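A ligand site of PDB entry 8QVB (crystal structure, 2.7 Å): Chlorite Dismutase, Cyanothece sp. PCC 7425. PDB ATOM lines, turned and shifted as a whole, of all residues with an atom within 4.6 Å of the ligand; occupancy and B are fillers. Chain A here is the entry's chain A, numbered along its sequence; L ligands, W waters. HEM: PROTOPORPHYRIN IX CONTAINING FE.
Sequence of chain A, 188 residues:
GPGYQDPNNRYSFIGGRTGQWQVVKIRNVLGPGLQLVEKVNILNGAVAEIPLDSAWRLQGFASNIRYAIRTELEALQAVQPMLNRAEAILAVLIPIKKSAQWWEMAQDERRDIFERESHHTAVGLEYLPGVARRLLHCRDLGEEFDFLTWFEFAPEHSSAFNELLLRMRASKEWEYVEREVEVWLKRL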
ATOM      1  N   ASN A  64      18.034 -10.053 -16.648  1.00  0.00           N
ATOM      2  CA  ASN A  64      17.080  -9.396 -15.788  1.00  0.00           C
ATOM      3  C   ASN A  64      17.758  -8.390 -14.854  1.00  0.00           C
ATOM      4  O   ASN A  64      18.956  -8.431 -14.567  1.00  0.00           O
ATOM      5  CB  ASN A  64      16.335 -10.455 -14.974  1.00  0.00           C
ATOM      6  CG  ASN A  64      17.269 -11.319 -14.151  1.00  0.00           C
ATOM      7  OD1 ASN A  64      17.941 -12.202 -14.689  1.00  0.00           O
ATOM      8  ND2 ASN A  64      17.308 -11.080 -12.841  1.00  0.00           N
ATOM      9  N   ILE A  65      16.927  -7.510 -14.305  1.00  0.00           N
ATOM     10  CA  ILE A  65      17.344  -6.470 -13.386  1.00  0.00           C
ATOM     11  C   ILE A  65      17.856  -7.108 -12.091  1.00  0.00           C
ATOM     12  O   ILE A  65      17.205  -8.011 -11.555  1.00  0.00           O
ATOM     13  CB  ILE A  65      16.148  -5.525 -13.171  1.00  0.00           C
ATOM     14  CG1 ILE A  65      15.952  -4.609 -14.379  1.00  0.00           C
ATOM     15  CG2 ILE A  65      16.284  -4.727 -11.877  1.00  0.00           C
ATOM     16  CD1 ILE A  65      17.054  -3.588 -14.574  1.00  0.00           C
ATOM     17  N   ARG A  66      18.996  -6.641 -11.585  1.00  0.00           N
ATOM     18  CA  ARG A  66      19.575  -7.162 -10.351  1.00  0.00           C
ATOM     19  C   ARG A  66      19.443  -6.205  -9.140  1.00  0.00           C
ATOM     20  O   ARG A  66      19.477  -6.704  -7.997  1.00  0.00           O
ATOM     21  CB  ARG A  66      21.058  -7.514 -10.575  1.00  0.00           C
ATOM     22  CG  ARG A  66      21.343  -8.280 -11.857  1.00  0.00           C
ATOM     23  CD  ARG A  66      20.629  -9.612 -11.957  1.00  0.00           C
ATOM     24  NE  ARG A  66      21.024 -10.437 -13.099  1.00  0.00           N
ATOM     25  CZ  ARG A  66      22.084 -11.233 -13.171  1.00  0.00           C
ATOM     26  NH1 ARG A  66      22.863 -11.449 -12.120  1.00  0.00           N
ATOM     27  NH2 ARG A  66      22.335 -11.867 -14.312  1.00  0.00           N
ATOM     28  N   TYR A  67      19.329  -4.872  -9.331  1.00  0.00           N
ATOM     29  CA  TYR A  67      19.388  -3.947  -8.197  1.00  0.00           C
ATOM     30  C   TYR A  67      18.250  -2.896  -8.214  1.00  0.00           C
ATOM     31  O   TYR A  67      17.688  -2.554  -7.162  1.00  0.00           O
ATOM     32  CB  TYR A  67      20.744  -3.235  -8.115  1.00  0.00           C
ATOM     33  CG  TYR A  67      21.924  -4.159  -7.830  1.00  0.00           C
ATOM     34  CD1 TYR A  67      22.117  -4.725  -6.581  1.00  0.00           C
ATOM     35  CD2 TYR A  67      22.815  -4.511  -8.850  1.00  0.00           C
ATOM     36  CE1 TYR A  67      23.177  -5.585  -6.339  1.00  0.00           C
ATOM     37  CE2 TYR A  67      23.859  -5.386  -8.618  1.00  0.00           C
ATOM     38  CZ  TYR A  67      24.045  -5.934  -7.359  1.00  0.00           C
ATOM     39  OH  TYR A  67      25.097  -6.801  -7.170  1.00  0.00           O
ATOM     40  N   ALA A  68      17.914  -2.373  -9.401  1.00  0.00           N
ATOM     41  CA  ALA A  68      16.899  -1.335  -9.519  1.00  0.00           C
ATOM     42  C   ALA A  68      15.550  -1.721  -8.934  1.00  0.00           C
ATOM     43  O   ALA A  68      15.004  -2.803  -9.180  1.00  0.00           O
ATOM     44  CB  ALA A  68      16.771  -0.986 -10.980  1.00  0.00           C
ATOM     45  N   LEU A  76      13.867   5.742 -14.971  1.00  0.00           N
ATOM     46  CA  LEU A  76      14.691   5.404 -16.117  1.00  0.00           C
ATOM     47  C   LEU A  76      13.851   5.382 -17.390  1.00  0.00           C
ATOM     48  O   LEU A  76      14.273   5.902 -18.401  1.00  0.00           O
ATOM     49  CB  LEU A  76      15.396   4.070 -15.868  1.00  0.00           C
ATOM     50  CG  LEU A  76      16.446   4.135 -14.756  1.00  0.00           C
ATOM     51  CD1 LEU A  76      16.754   2.752 -14.198  1.00  0.00           C
ATOM     52  CD2 LEU A  76      17.729   4.798 -15.241  1.00  0.00           C
ATOM     53  N   ILE A  94      32.908  -0.273 -22.262  1.00  0.00           N
ATOM     54  CA  ILE A  94      33.707  -0.264 -21.041  1.00  0.00           C
ATOM     55  C   ILE A  94      33.515  -1.577 -20.315  1.00  0.00           C
ATOM     56  O   ILE A  94      32.543  -1.735 -19.574  1.00  0.00           O
ATOM     57  CB  ILE A  94      33.401   0.932 -20.121  1.00  0.00           C
ATOM     58  CG1 ILE A  94      33.455   2.259 -20.862  1.00  0.00           C
ATOM     59  CG2 ILE A  94      34.349   0.942 -18.916  1.00  0.00           C
ATOM     60  CD1 ILE A  94      33.045   3.442 -20.028  1.00  0.00           C
ATOM     61  N   ILE A  96      34.337  -4.158 -17.306  1.00  0.00           N
ATOM     62  CA  ILE A  96      34.568  -3.971 -15.896  1.00  0.00           C
ATOM     63  C   ILE A  96      34.628  -5.338 -15.227  1.00  0.00           C
ATOM     64  O   ILE A  96      33.773  -6.184 -15.483  1.00  0.00           O
ATOM     65  CB  ILE A  96      33.447  -3.119 -15.279  1.00  0.00           C
ATOM     66  CG1 ILE A  96      33.594  -1.647 -15.674  1.00  0.00           C
ATOM     67  CG2 ILE A  96      33.388  -3.286 -13.767  1.00  0.00           C
ATOM     68  CD1 ILE A  96      32.302  -0.892 -15.613  1.00  0.00           C
ATOM     69  N   LYS A  98      34.776  -6.727 -11.139  1.00  0.00           N
ATOM     70  CA  LYS A  98      34.714  -6.415  -9.720  1.00  0.00           C
ATOM     71  C   LYS A  98      35.445  -7.502  -8.924  1.00  0.00           C
ATOM     72  O   LYS A  98      35.695  -8.573  -9.454  1.00  0.00           O
ATOM     73  CB  LYS A  98      33.255  -6.267  -9.323  1.00  0.00           C
ATOM     74  CG  LYS A  98      32.534  -5.079  -9.918  1.00  0.00           C
ATOM     75  CD  LYS A  98      31.267  -4.729  -9.189  1.00  0.00           C
ATOM     76  CE  LYS A  98      30.535  -3.528  -9.787  1.00  0.00           C
ATOM     77  NZ  LYS A  98      29.216  -3.269  -9.140  1.00  0.00           N
ATOM     78  N   TRP A 102      33.624  -8.289  -3.535  1.00  0.00           N
ATOM     79  CA  TRP A 102      32.316  -7.829  -3.981  1.00  0.00           C
ATOM     80  C   TRP A 102      31.377  -9.020  -4.181  1.00  0.00           C
ATOM     81  O   TRP A 102      30.271  -9.024  -3.648  1.00  0.00           O
ATOM     82  CB  TRP A 102      32.414  -7.019  -5.279  1.00  0.00           C
ATOM     83  CG  TRP A 102      31.082  -6.695  -5.908  1.00  0.00           C
ATOM     84  CD1 TRP A 102      30.487  -7.341  -6.951  1.00  0.00           C
ATOM     85  CD2 TRP A 102      30.193  -5.605  -5.555  1.00  0.00           C
ATOM     86  NE1 TRP A 102      29.287  -6.768  -7.247  1.00  0.00           N
ATOM     87  CE2 TRP A 102      29.079  -5.692  -6.417  1.00  0.00           C
ATOM     88  CE3 TRP A 102      30.226  -4.590  -4.606  1.00  0.00           C
ATOM     89  CZ2 TRP A 102      28.015  -4.799  -6.362  1.00  0.00           C
ATOM     90  CZ3 TRP A 102      29.173  -3.688  -4.553  1.00  0.00           C
ATOM     91  CH2 TRP A 102      28.087  -3.798  -5.424  1.00  0.00           C
ATOM     92  N   PHE A 114      25.779   0.031  -3.933  1.00  0.00           N
ATOM     93  CA  PHE A 114      25.447   0.429  -5.295  1.00  0.00           C
ATOM     94  C   PHE A 114      24.597   1.713  -5.303  1.00  0.00           C
ATOM     95  O   PHE A 114      24.881   2.630  -6.083  1.00  0.00           O
ATOM     96  CB  PHE A 114      24.788  -0.742  -6.032  1.00  0.00           C
ATOM     97  CG  PHE A 114      24.310  -0.418  -7.418  1.00  0.00           C
ATOM     98  CD1 PHE A 114      25.185  -0.430  -8.490  1.00  0.00           C
ATOM     99  CD2 PHE A 114      22.985  -0.068  -7.647  1.00  0.00           C
ATOM    100  CE1 PHE A 114      24.749  -0.107  -9.772  1.00  0.00           C
ATOM    101  CE2 PHE A 114      22.559   0.264  -8.930  1.00  0.00           C
ATOM    102  CZ  PHE A 114      23.437   0.250  -9.986  1.00  0.00           C
ATOM    103  N   HIS A 120      24.411   5.235  -7.811  1.00  0.00           N
ATOM    104  CA  HIS A 120      24.694   4.893  -9.199  1.00  0.00           C
ATOM    105  C   HIS A 120      23.567   5.353 -10.126  1.00  0.00           C
ATOM    106  O   HIS A 120      23.814   5.972 -11.141  1.00  0.00           O
ATOM    107  CB  HIS A 120      24.998   3.401  -9.343  1.00  0.00           C
ATOM    108  CG  HIS A 120      25.397   2.962 -10.721  1.00  0.00           C
ATOM    109  ND1 HIS A 120      26.625   2.413 -10.963  1.00  0.00           N
ATOM    110  CD2 HIS A 120      24.741   2.947 -11.915  1.00  0.00           C
ATOM    111  CE1 HIS A 120      26.715   2.099 -12.246  1.00  0.00           C
ATOM    112  NE2 HIS A 120      25.595   2.423 -12.857  1.00  0.00           N
ATOM    113  N   THR A 121      22.321   5.066  -9.773  1.00  0.00           N
ATOM    114  CA  THR A 121      21.199   5.358 -10.643  1.00  0.00           C
ATOM    115  C   THR A 121      20.876   6.845 -10.627  1.00  0.00           C
ATOM    116  O   THR A 121      20.697   7.455 -11.672  1.00  0.00           O
ATOM    117  CB  THR A 121      19.993   4.487 -10.277  1.00  0.00           C
ATOM    118  OG1 THR A 121      20.371   3.108 -10.222  1.00  0.00           O
ATOM    119  CG2 THR A 121      18.865   4.621 -11.265  1.00  0.00           C
ATOM    120  N   GLY A 124      23.589   8.571 -12.626  1.00  0.00           N
ATOM    121  CA  GLY A 124      23.496   8.250 -14.041  1.00  0.00           C
ATOM    122  C   GLY A 124      22.324   8.941 -14.729  1.00  0.00           C
ATOM    123  O   GLY A 124      22.456   9.363 -15.877  1.00  0.00           O
ATOM    124  N   LEU A 125      21.200   9.056 -14.012  1.00  0.00           N
ATOM    125  CA  LEU A 125      20.005   9.759 -14.480  1.00  0.00           C
ATOM    126  C   LEU A 125      20.268  11.220 -14.859  1.00  0.00           C
ATOM    127  O   LEU A 125      19.580  11.789 -15.688  1.00  0.00           O
ATOM    128  CB  LEU A 125      18.918   9.679 -13.400  1.00  0.00           C
ATOM    129  CG  LEU A 125      17.828   8.650 -13.649  1.00  0.00           C
ATOM    130  CD1 LEU A 125      16.864   8.594 -12.481  1.00  0.00           C
ATOM    131  CD2 LEU A 125      17.077   8.951 -14.935  1.00  0.00           C
ATOM    132  N   LEU A 128      20.983  11.523 -18.699  1.00  0.00           N
ATOM    133  CA  LEU A 128      19.953  11.108 -19.642  1.00  0.00           C
ATOM    134  C   LEU A 128      19.098  12.321 -19.990  1.00  0.00           C
ATOM    135  O   LEU A 128      18.936  13.141 -19.098  1.00  0.00           O
ATOM    136  CB  LEU A 128      19.112  10.007 -18.996  1.00  0.00           C
ATOM    137  CG  LEU A 128      19.532   8.590 -19.348  1.00  0.00           C
ATOM    138  CD1 LEU A 128      21.021   8.412 -19.183  1.00  0.00           C
ATOM    139  CD2 LEU A 128      18.777   7.590 -18.501  1.00  0.00           C
ATOM    140  N   VAL A 131      22.817  10.393 -23.073  1.00  0.00           N
ATOM    141  CA  VAL A 131      23.500   9.092 -23.155  1.00  0.00           C
ATOM    142  C   VAL A 131      22.530   7.902 -23.211  1.00  0.00           C
ATOM    143  O   VAL A 131      21.744   7.657 -22.295  1.00  0.00           O
ATOM    144  CB  VAL A 131      24.458   8.888 -21.964  1.00  0.00           C
ATOM    145  CG1 VAL A 131      25.198   7.569 -22.097  1.00  0.00           C
ATOM    146  CG2 VAL A 131      25.439  10.048 -21.801  1.00  0.00           C
ATOM    147  N   ARG A 133      22.507   3.577 -23.267  1.00  0.00           N
ATOM    148  CA  ARG A 133      23.353   2.573 -22.631  1.00  0.00           C
ATOM    149  C   ARG A 133      22.816   1.155 -22.858  1.00  0.00           C
ATOM    150  O   ARG A 133      21.634   0.954 -23.069  1.00  0.00           O
ATOM    151  CB  ARG A 133      23.468   2.870 -21.134  1.00  0.00           C
ATOM    152  CG  ARG A 133      22.202   2.569 -20.338  1.00  0.00           C
ATOM    153  CD  ARG A 133      22.274   3.085 -18.902  1.00  0.00           C
ATOM    154  NE  ARG A 133      21.225   2.480 -18.093  1.00  0.00           N
ATOM    155  CZ  ARG A 133      19.928   2.780 -18.150  1.00  0.00           C
ATOM    156  NH1 ARG A 133      19.496   3.788 -18.878  1.00  0.00           N
ATOM    157  NH2 ARG A 133      19.053   2.072 -17.457  1.00  0.00           N
ATOM    158  N   LEU A 135      23.637  -2.844 -21.011  1.00  0.00           N
ATOM    159  CA  LEU A 135      24.405  -3.576 -20.023  1.00  0.00           C
ATOM    160  C   LEU A 135      24.360  -5.070 -20.297  1.00  0.00           C
ATOM    161  O   LEU A 135      23.296  -5.666 -20.496  1.00  0.00           O
ATOM    162  CB  LEU A 135      23.860  -3.292 -18.624  1.00  0.00           C
ATOM    163  CG  LEU A 135      24.458  -4.147 -17.517  1.00  0.00           C
ATOM    164  CD1 LEU A 135      25.925  -3.857 -17.353  1.00  0.00           C
ATOM    165  CD2 LEU A 135      23.737  -3.934 -16.200  1.00  0.00           C
ATOM    166  N   HIS A 137      26.189  -8.909 -19.027  1.00  0.00           N
ATOM    167  CA  HIS A 137      26.799  -9.689 -17.967  1.00  0.00           C
ATOM    168  C   HIS A 137      27.674 -10.776 -18.585  1.00  0.00           C
ATOM    169  O   HIS A 137      27.260 -11.355 -19.607  1.00  0.00           O
ATOM    170  CB  HIS A 137      25.675 -10.346 -17.148  1.00  0.00           C
ATOM    171  CG  HIS A 137      24.736  -9.357 -16.533  1.00  0.00           C
ATOM    172  ND1 HIS A 137      24.782  -9.035 -15.184  1.00  0.00           N
ATOM    173  CD2 HIS A 137      23.751  -8.632 -17.080  1.00  0.00           C
ATOM    174  CE1 HIS A 137      23.825  -8.152 -14.946  1.00  0.00           C
ATOM    175  NE2 HIS A 137      23.197  -7.872 -16.084  1.00  0.00           N
ATOM    176  N   PHE A 147      31.569  -7.594 -16.717  1.00  0.00           N
ATOM    177  CA  PHE A 147      30.523  -6.843 -17.409  1.00  0.00           C
ATOM    178  C   PHE A 147      31.068  -6.149 -18.642  1.00  0.00           C
ATOM    179  O   PHE A 147      32.212  -5.728 -18.678  1.00  0.00           O
ATOM    180  CB  PHE A 147      29.887  -5.725 -16.567  1.00  0.00           C
ATOM    181  CG  PHE A 147      29.409  -6.123 -15.190  1.00  0.00           C
ATOM    182  CD1 PHE A 147      28.219  -6.794 -15.013  1.00  0.00           C
ATOM    183  CD2 PHE A 147      30.167  -5.829 -14.076  1.00  0.00           C
ATOM    184  CE1 PHE A 147      27.776  -7.161 -13.747  1.00  0.00           C
ATOM    185  CE2 PHE A 147      29.733  -6.195 -12.806  1.00  0.00           C
ATOM    186  CZ  PHE A 147      28.551  -6.877 -12.644  1.00  0.00           C
ATOM    187  N   THR A 149      29.826  -2.768 -20.668  1.00  0.00           N
ATOM    188  CA  THR A 149      28.884  -1.665 -20.646  1.00  0.00           C
ATOM    189  C   THR A 149      29.063  -0.925 -21.959  1.00  0.00           C
ATOM    190  O   THR A 149      30.156  -0.886 -22.496  1.00  0.00           O
ATOM    191  CB  THR A 149      29.066  -0.808 -19.398  1.00  0.00           C
ATOM    192  OG1 THR A 149      30.313  -0.119 -19.437  1.00  0.00           O
ATOM    193  CG2 THR A 149      28.957  -1.643 -18.141  1.00  0.00           C
ATOM    194  N   PHE A 151      27.739   2.608 -24.163  1.00  0.00           N
ATOM    195  CA  PHE A 151      27.205   3.963 -24.108  1.00  0.00           C
ATOM    196  C   PHE A 151      27.357   4.610 -25.461  1.00  0.00           C
ATOM    197  O   PHE A 151      28.426   4.497 -26.076  1.00  0.00           O
ATOM    198  CB  PHE A 151      27.936   4.818 -23.078  1.00  0.00           C
ATOM    199  CG  PHE A 151      28.030   4.148 -21.753  1.00  0.00           C
ATOM    200  CD1 PHE A 151      26.952   4.190 -20.876  1.00  0.00           C
ATOM    201  CD2 PHE A 151      29.106   3.354 -21.442  1.00  0.00           C
ATOM    202  CE1 PHE A 151      27.012   3.510 -19.670  1.00  0.00           C
ATOM    203  CE2 PHE A 151      29.144   2.644 -20.252  1.00  0.00           C
ATOM    204  CZ  PHE A 151      28.101   2.733 -19.365  1.00  0.00           C
ATOM    205  N   PHE A 161      29.740  13.044 -20.724  1.00  0.00           N
ATOM    206  CA  PHE A 161      30.052  11.643 -20.514  1.00  0.00           C
ATOM    207  C   PHE A 161      31.357  11.507 -19.726  1.00  0.00           C
ATOM    208  O   PHE A 161      31.428  10.693 -18.805  1.00  0.00           O
ATOM    209  CB  PHE A 161      30.103  10.846 -21.831  1.00  0.00           C
ATOM    210  CG  PHE A 161      30.293   9.361 -21.597  1.00  0.00           C
ATOM    211  CD1 PHE A 161      29.260   8.593 -21.079  1.00  0.00           C
ATOM    212  CD2 PHE A 161      31.527   8.769 -21.792  1.00  0.00           C
ATOM    213  CE1 PHE A 161      29.450   7.243 -20.782  1.00  0.00           C
ATOM    214  CE2 PHE A 161      31.717   7.416 -21.520  1.00  0.00           C
ATOM    215  CZ  PHE A 161      30.682   6.662 -20.999  1.00  0.00           C
ATOM    216  N   LEU A 164      30.703  12.201 -16.184  1.00  0.00           N
ATOM    217  CA  LEU A 164      30.075  11.040 -15.557  1.00  0.00           C
ATOM    218  C   LEU A 164      31.103   9.958 -15.185  1.00  0.00           C
ATOM    219  O   LEU A 164      31.069   9.456 -14.062  1.00  0.00           O
ATOM    220  CB  LEU A 164      28.952  10.522 -16.461  1.00  0.00           C
ATOM    221  CG  LEU A 164      28.393   9.129 -16.126  1.00  0.00           C
ATOM    222  CD1 LEU A 164      27.613   9.121 -14.815  1.00  0.00           C
ATOM    223  CD2 LEU A 164      27.526   8.614 -17.259  1.00  0.00           C
ATOM    224  N   LEU A 165      32.051   9.624 -16.067  1.00  0.00           N
ATOM    225  CA  LEU A 165      33.038   8.589 -15.763  1.00  0.00           C
ATOM    226  C   LEU A 165      33.790   8.900 -14.491  1.00  0.00           C
ATOM    227  O   LEU A 165      34.071   8.015 -13.703  1.00  0.00           O
ATOM    228  CB  LEU A 165      34.067   8.482 -16.887  1.00  0.00           C
ATOM    229  CG  LEU A 165      33.606   7.804 -18.171  1.00  0.00           C
ATOM    230  CD1 LEU A 165      34.720   7.890 -19.214  1.00  0.00           C
ATOM    231  CD2 LEU A 165      33.207   6.343 -17.958  1.00  0.00           C
ATOM    232  N   MET A 168      31.651   8.387 -11.279  1.00  0.00           N
ATOM    233  CA  MET A 168      31.412   6.992 -10.921  1.00  0.00           C
ATOM    234  C   MET A 168      32.659   6.440 -10.239  1.00  0.00           C
ATOM    235  O   MET A 168      32.564   5.748  -9.226  1.00  0.00           O
ATOM    236  CB  MET A 168      31.091   6.173 -12.163  1.00  0.00           C
ATOM    237  CG  MET A 168      29.721   6.454 -12.795  1.00  0.00           C
ATOM    238  SD  MET A 168      28.387   5.857 -11.767  1.00  0.00           S
ATOM    239  CE  MET A 168      27.037   5.798 -12.948  1.00  0.00           C
ATOM    240  N   GLU A 173      31.285   2.241  -4.739  1.00  0.00           N
ATOM    241  CA  GLU A 173      31.186   1.123  -5.661  1.00  0.00           C
ATOM    242  C   GLU A 173      32.530   0.844  -6.333  1.00  0.00           C
ATOM    243  O   GLU A 173      32.932  -0.308  -6.442  1.00  0.00           O
ATOM    244  CB  GLU A 173      30.118   1.369  -6.739  1.00  0.00           C
ATOM    245  CG  GLU A 173      29.809   0.152  -7.607  1.00  0.00           C
ATOM    246  CD  GLU A 173      28.793   0.378  -8.723  1.00  0.00           C
ATOM    247  OE1 GLU A 173      28.368   1.540  -8.888  1.00  0.00           O
ATOM    248  OE2 GLU A 173      28.423  -0.612  -9.438  1.00  0.00           O
ATOM    249  N   TRP A 174      33.211   1.903  -6.805  1.00  0.00           N
ATOM    250  CA  TRP A 174      34.369   1.708  -7.676  1.00  0.00           C
ATOM    251  C   TRP A 174      35.603   1.232  -6.935  1.00  0.00           C
ATOM    252  O   TRP A 174      36.587   0.911  -7.579  1.00  0.00           O
ATOM    253  CB  TRP A 174      34.680   2.946  -8.526  1.00  0.00           C
ATOM    254  CG  TRP A 174      34.522   2.660 -10.000  1.00  0.00           C
ATOM    255  CD1 TRP A 174      35.525   2.484 -10.900  1.00  0.00           C
ATOM    256  CD2 TRP A 174      33.282   2.516 -10.739  1.00  0.00           C
ATOM    257  NE1 TRP A 174      35.016   2.226 -12.137  1.00  0.00           N
ATOM    258  CE2 TRP A 174      33.643   2.253 -12.076  1.00  0.00           C
ATOM    259  CE3 TRP A 174      31.928   2.599 -10.415  1.00  0.00           C
ATOM    260  CZ2 TRP A 174      32.681   2.042 -13.076  1.00  0.00           C
ATOM    261  CZ3 TRP A 174      30.980   2.417 -11.402  1.00  0.00           C
ATOM    262  CH2 TRP A 174      31.355   2.132 -12.715  1.00  0.00           C
ATOM    263  N   GLU A 180      39.458  -2.358 -15.657  1.00  0.00           N
ATOM    264  CA  GLU A 180      38.625  -1.440 -16.425  1.00  0.00           C
ATOM    265  C   GLU A 180      39.394  -0.974 -17.657  1.00  0.00           C
ATOM    266  O   GLU A 180      40.592  -0.713 -17.574  1.00  0.00           O
ATOM    267  CB  GLU A 180      38.222  -0.269 -15.552  1.00  0.00           C
ATOM    268  CG  GLU A 180      37.244   0.669 -16.195  1.00  0.00           C
ATOM    269  CD  GLU A 180      36.700   1.730 -15.250  1.00  0.00           C
ATOM    270  OE1 GLU A 180      37.113   1.732 -14.026  1.00  0.00           O
ATOM    271  OE2 GLU A 180      35.872   2.554 -15.732  1.00  0.00           O
HETATM  272  CHA HEM L   1      24.301  -1.228 -13.521  1.00  0.00           C
HETATM  273  CHB HEM L   1      22.084   2.856 -14.676  1.00  0.00           C
HETATM  274  CHC HEM L   1      26.183   4.683 -16.379  1.00  0.00           C
HETATM  275  CHD HEM L   1      28.466   0.704 -14.929  1.00  0.00           C
HETATM  276  C1A HEM L   1      23.371  -0.235 -13.670  1.00  0.00           C
HETATM  277  C2A HEM L   1      22.042  -0.348 -13.177  1.00  0.00           C
HETATM  278  C3A HEM L   1      21.424   0.814 -13.524  1.00  0.00           C
HETATM  279  C4A HEM L   1      22.357   1.617 -14.201  1.00  0.00           C
HETATM  280  CMA HEM L   1      19.995   1.183 -13.204  1.00  0.00           C
HETATM  281  CAA HEM L   1      21.419  -1.484 -12.417  1.00  0.00           C
HETATM  282  CBA HEM L   1      20.949  -2.605 -13.345  1.00  0.00           C
HETATM  283  CGA HEM L   1      20.255  -3.727 -12.580  1.00  0.00           C
HETATM  284  O1A HEM L   1      20.420  -4.871 -13.022  1.00  0.00           O
HETATM  285  O2A HEM L   1      19.535  -3.563 -11.549  1.00  0.00           O
HETATM  286  C1B HEM L   1      23.009   3.680 -15.265  1.00  0.00           C
HETATM  287  C2B HEM L   1      22.636   4.903 -15.810  1.00  0.00           C
HETATM  288  C3B HEM L   1      23.766   5.450 -16.292  1.00  0.00           C
HETATM  289  C4B HEM L   1      24.858   4.502 -16.049  1.00  0.00           C
HETATM  290  CMB HEM L   1      21.278   5.549 -15.920  1.00  0.00           C
HETATM  291  CAB HEM L   1      23.726   6.685 -17.070  1.00  0.00           C
HETATM  292  CBB HEM L   1      24.603   6.829 -18.065  1.00  0.00           C
HETATM  293  C1C HEM L   1      27.196   3.786 -16.095  1.00  0.00           C
HETATM  294  C2C HEM L   1      28.567   3.917 -16.417  1.00  0.00           C
HETATM  295  C3C HEM L   1      29.186   2.762 -16.021  1.00  0.00           C
HETATM  296  C4C HEM L   1      28.199   1.954 -15.422  1.00  0.00           C
HETATM  297  CMC HEM L   1      29.244   5.055 -17.123  1.00  0.00           C
HETATM  298  CAC HEM L   1      30.593   2.383 -16.118  1.00  0.00           C
HETATM  299  CBC HEM L   1      31.571   3.158 -16.563  1.00  0.00           C
HETATM  300  C1D HEM L   1      27.478  -0.141 -14.465  1.00  0.00           C
HETATM  301  C2D HEM L   1      27.754  -1.529 -14.055  1.00  0.00           C
HETATM  302  C3D HEM L   1      26.597  -2.059 -13.666  1.00  0.00           C
HETATM  303  C4D HEM L   1      25.613  -1.015 -13.880  1.00  0.00           C
HETATM  304  CMD HEM L   1      29.095  -2.243 -14.038  1.00  0.00           C
HETATM  305  CAD HEM L   1      26.392  -3.442 -13.166  1.00  0.00           C
HETATM  306  CBD HEM L   1      26.596  -3.487 -11.657  1.00  0.00           C
HETATM  307  CGD HEM L   1      26.386  -4.887 -11.092  1.00  0.00           C
HETATM  308  O1D HEM L   1      25.485  -5.658 -11.562  1.00  0.00           O
HETATM  309  O2D HEM L   1      27.149  -5.239 -10.166  1.00  0.00           O
HETATM  310  NA  HEM L   1      23.548   0.990 -14.313  1.00  0.00           N
HETATM  311  NB  HEM L   1      24.300   3.474 -15.441  1.00  0.00           N
HETATM  312  NC  HEM L   1      27.016   2.625 -15.485  1.00  0.00           N
HETATM  313  ND  HEM L   1      26.180   0.126 -14.364  1.00  0.00           N
HETATM  314 FE   HEM L   1      25.307   1.780 -14.813  1.00  0.00          FE
HETATM  315  O   HOH W   1      24.394   0.648 -17.363  1.00  0.00           O
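The backbone NH (N) of His 120 sits at hydrogen-bond distance from the backbone carbonyl oxygen (O) of Phe 114 (3.2 Å). The side-chain carboxylate (OE1) of Glu 173 lies within hydrogen-bond range of a ring nitrogen (ND1) of His 120 (2.8 Å). The guanidinium group (NE) of Arg 66 sits at hydrogen-bond distance from the backbone carbonyl oxygen (O) of Asn 64, at 3.2 Å. The side-chain carboxylate (OE2) of Glu 173 lies within salt-bridge range of the side-chain amino group (NZ) of Lys 98 (2.8 Å). The backbone NH of Phe 147 sits at hydrogen-bond distance from the backbone carbonyl oxygen of Ile 96 (2.9 Å). NE1 of Trp 174 sits at hydrogen-bond distance from OE1 of Glu 180 (2.9 Å). OG1 of Thr 149 lies within hydrogen-bond range of O of Ile 94 (2.8 Å).
NE2 of His 120 is bound to FE of the ligand, at 2.1 Å. The backbone NH (N) of Tyr 67 sits at hydrogen-bond distance from an oxygen (O2A) of the ligand (2.6 Å). O1A of the ligand sits at hydrogen-bond distance from N of Arg 66 (2.7 Å). N of Ala 68 is in hydrogen-bond range of O2A of the ligand, 2.9 Å away. The side-chain amino group (NZ) of Lys 98 lies within salt-bridge range of an oxygen (O2D) of the ligand (3.0 Å).
Ile 65 touches the ligand (CG2 to O2A, 3.5 Å). CD2 of Leu 76 touches CMB of the ligand, 3.7 Å away. Ile 94 touches the ligand. Ile 96 touches the ligand (CD1 to CAC, 3.7 Å). CZ2 of Trp 102 touches O2D of the ligand (3.9 Å). Phe 114 touches the ligand. Thr 121 touches the ligand. Gly 124 touches the ligand. Leu 125 touches the ligand (N to CMB, 3.99 Å). Leu 128 touches the ligand (CD1 to CAB, 3.8 Å). NE of Arg 133 touches CHB of the ligand, at 3.5 Å. CD2 of Leu 135 touches CHA of the ligand (3.8 Å). Phe 147 touches the ligand (CZ to O2D, 3.3 Å). Phe 151 touches the ligand. Leu 164 touches the ligand (CD2 to CBB, 3.5 Å). Leu 165 touches the ligand (CD2 to CBC, 3.8 Å). Met 168 touches the ligand (CE to CHC, 3.7 Å). Trp 174 touches the ligand (CH2 to CAC, 3.5 Å). Hydrophobic or aromatic side chains within 4 Å of the ligand: Ile 65, Tyr 67, Ala 68, Leu 76, Ile 94, Ile 96, Trp 102, Phe 114, His 120, Leu 128, Leu 135, Phe 147, Phe 151, Leu 164, Leu 165, Met 168 and Trp 174. 23 residues have an atom within 4 Å of the ligand: Ile 65, Arg 66, Tyr 67, Ala 68, Leu 76, Ile 94, Ile 96, Lys 98, Trp 102, Phe 114, His 120, Thr 121, Gly 124, Leu 125, Leu 128, Arg 133, Leu 135, Phe 147, Phe 151, Leu 164, Leu 165, Met 168 and Trp 174.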
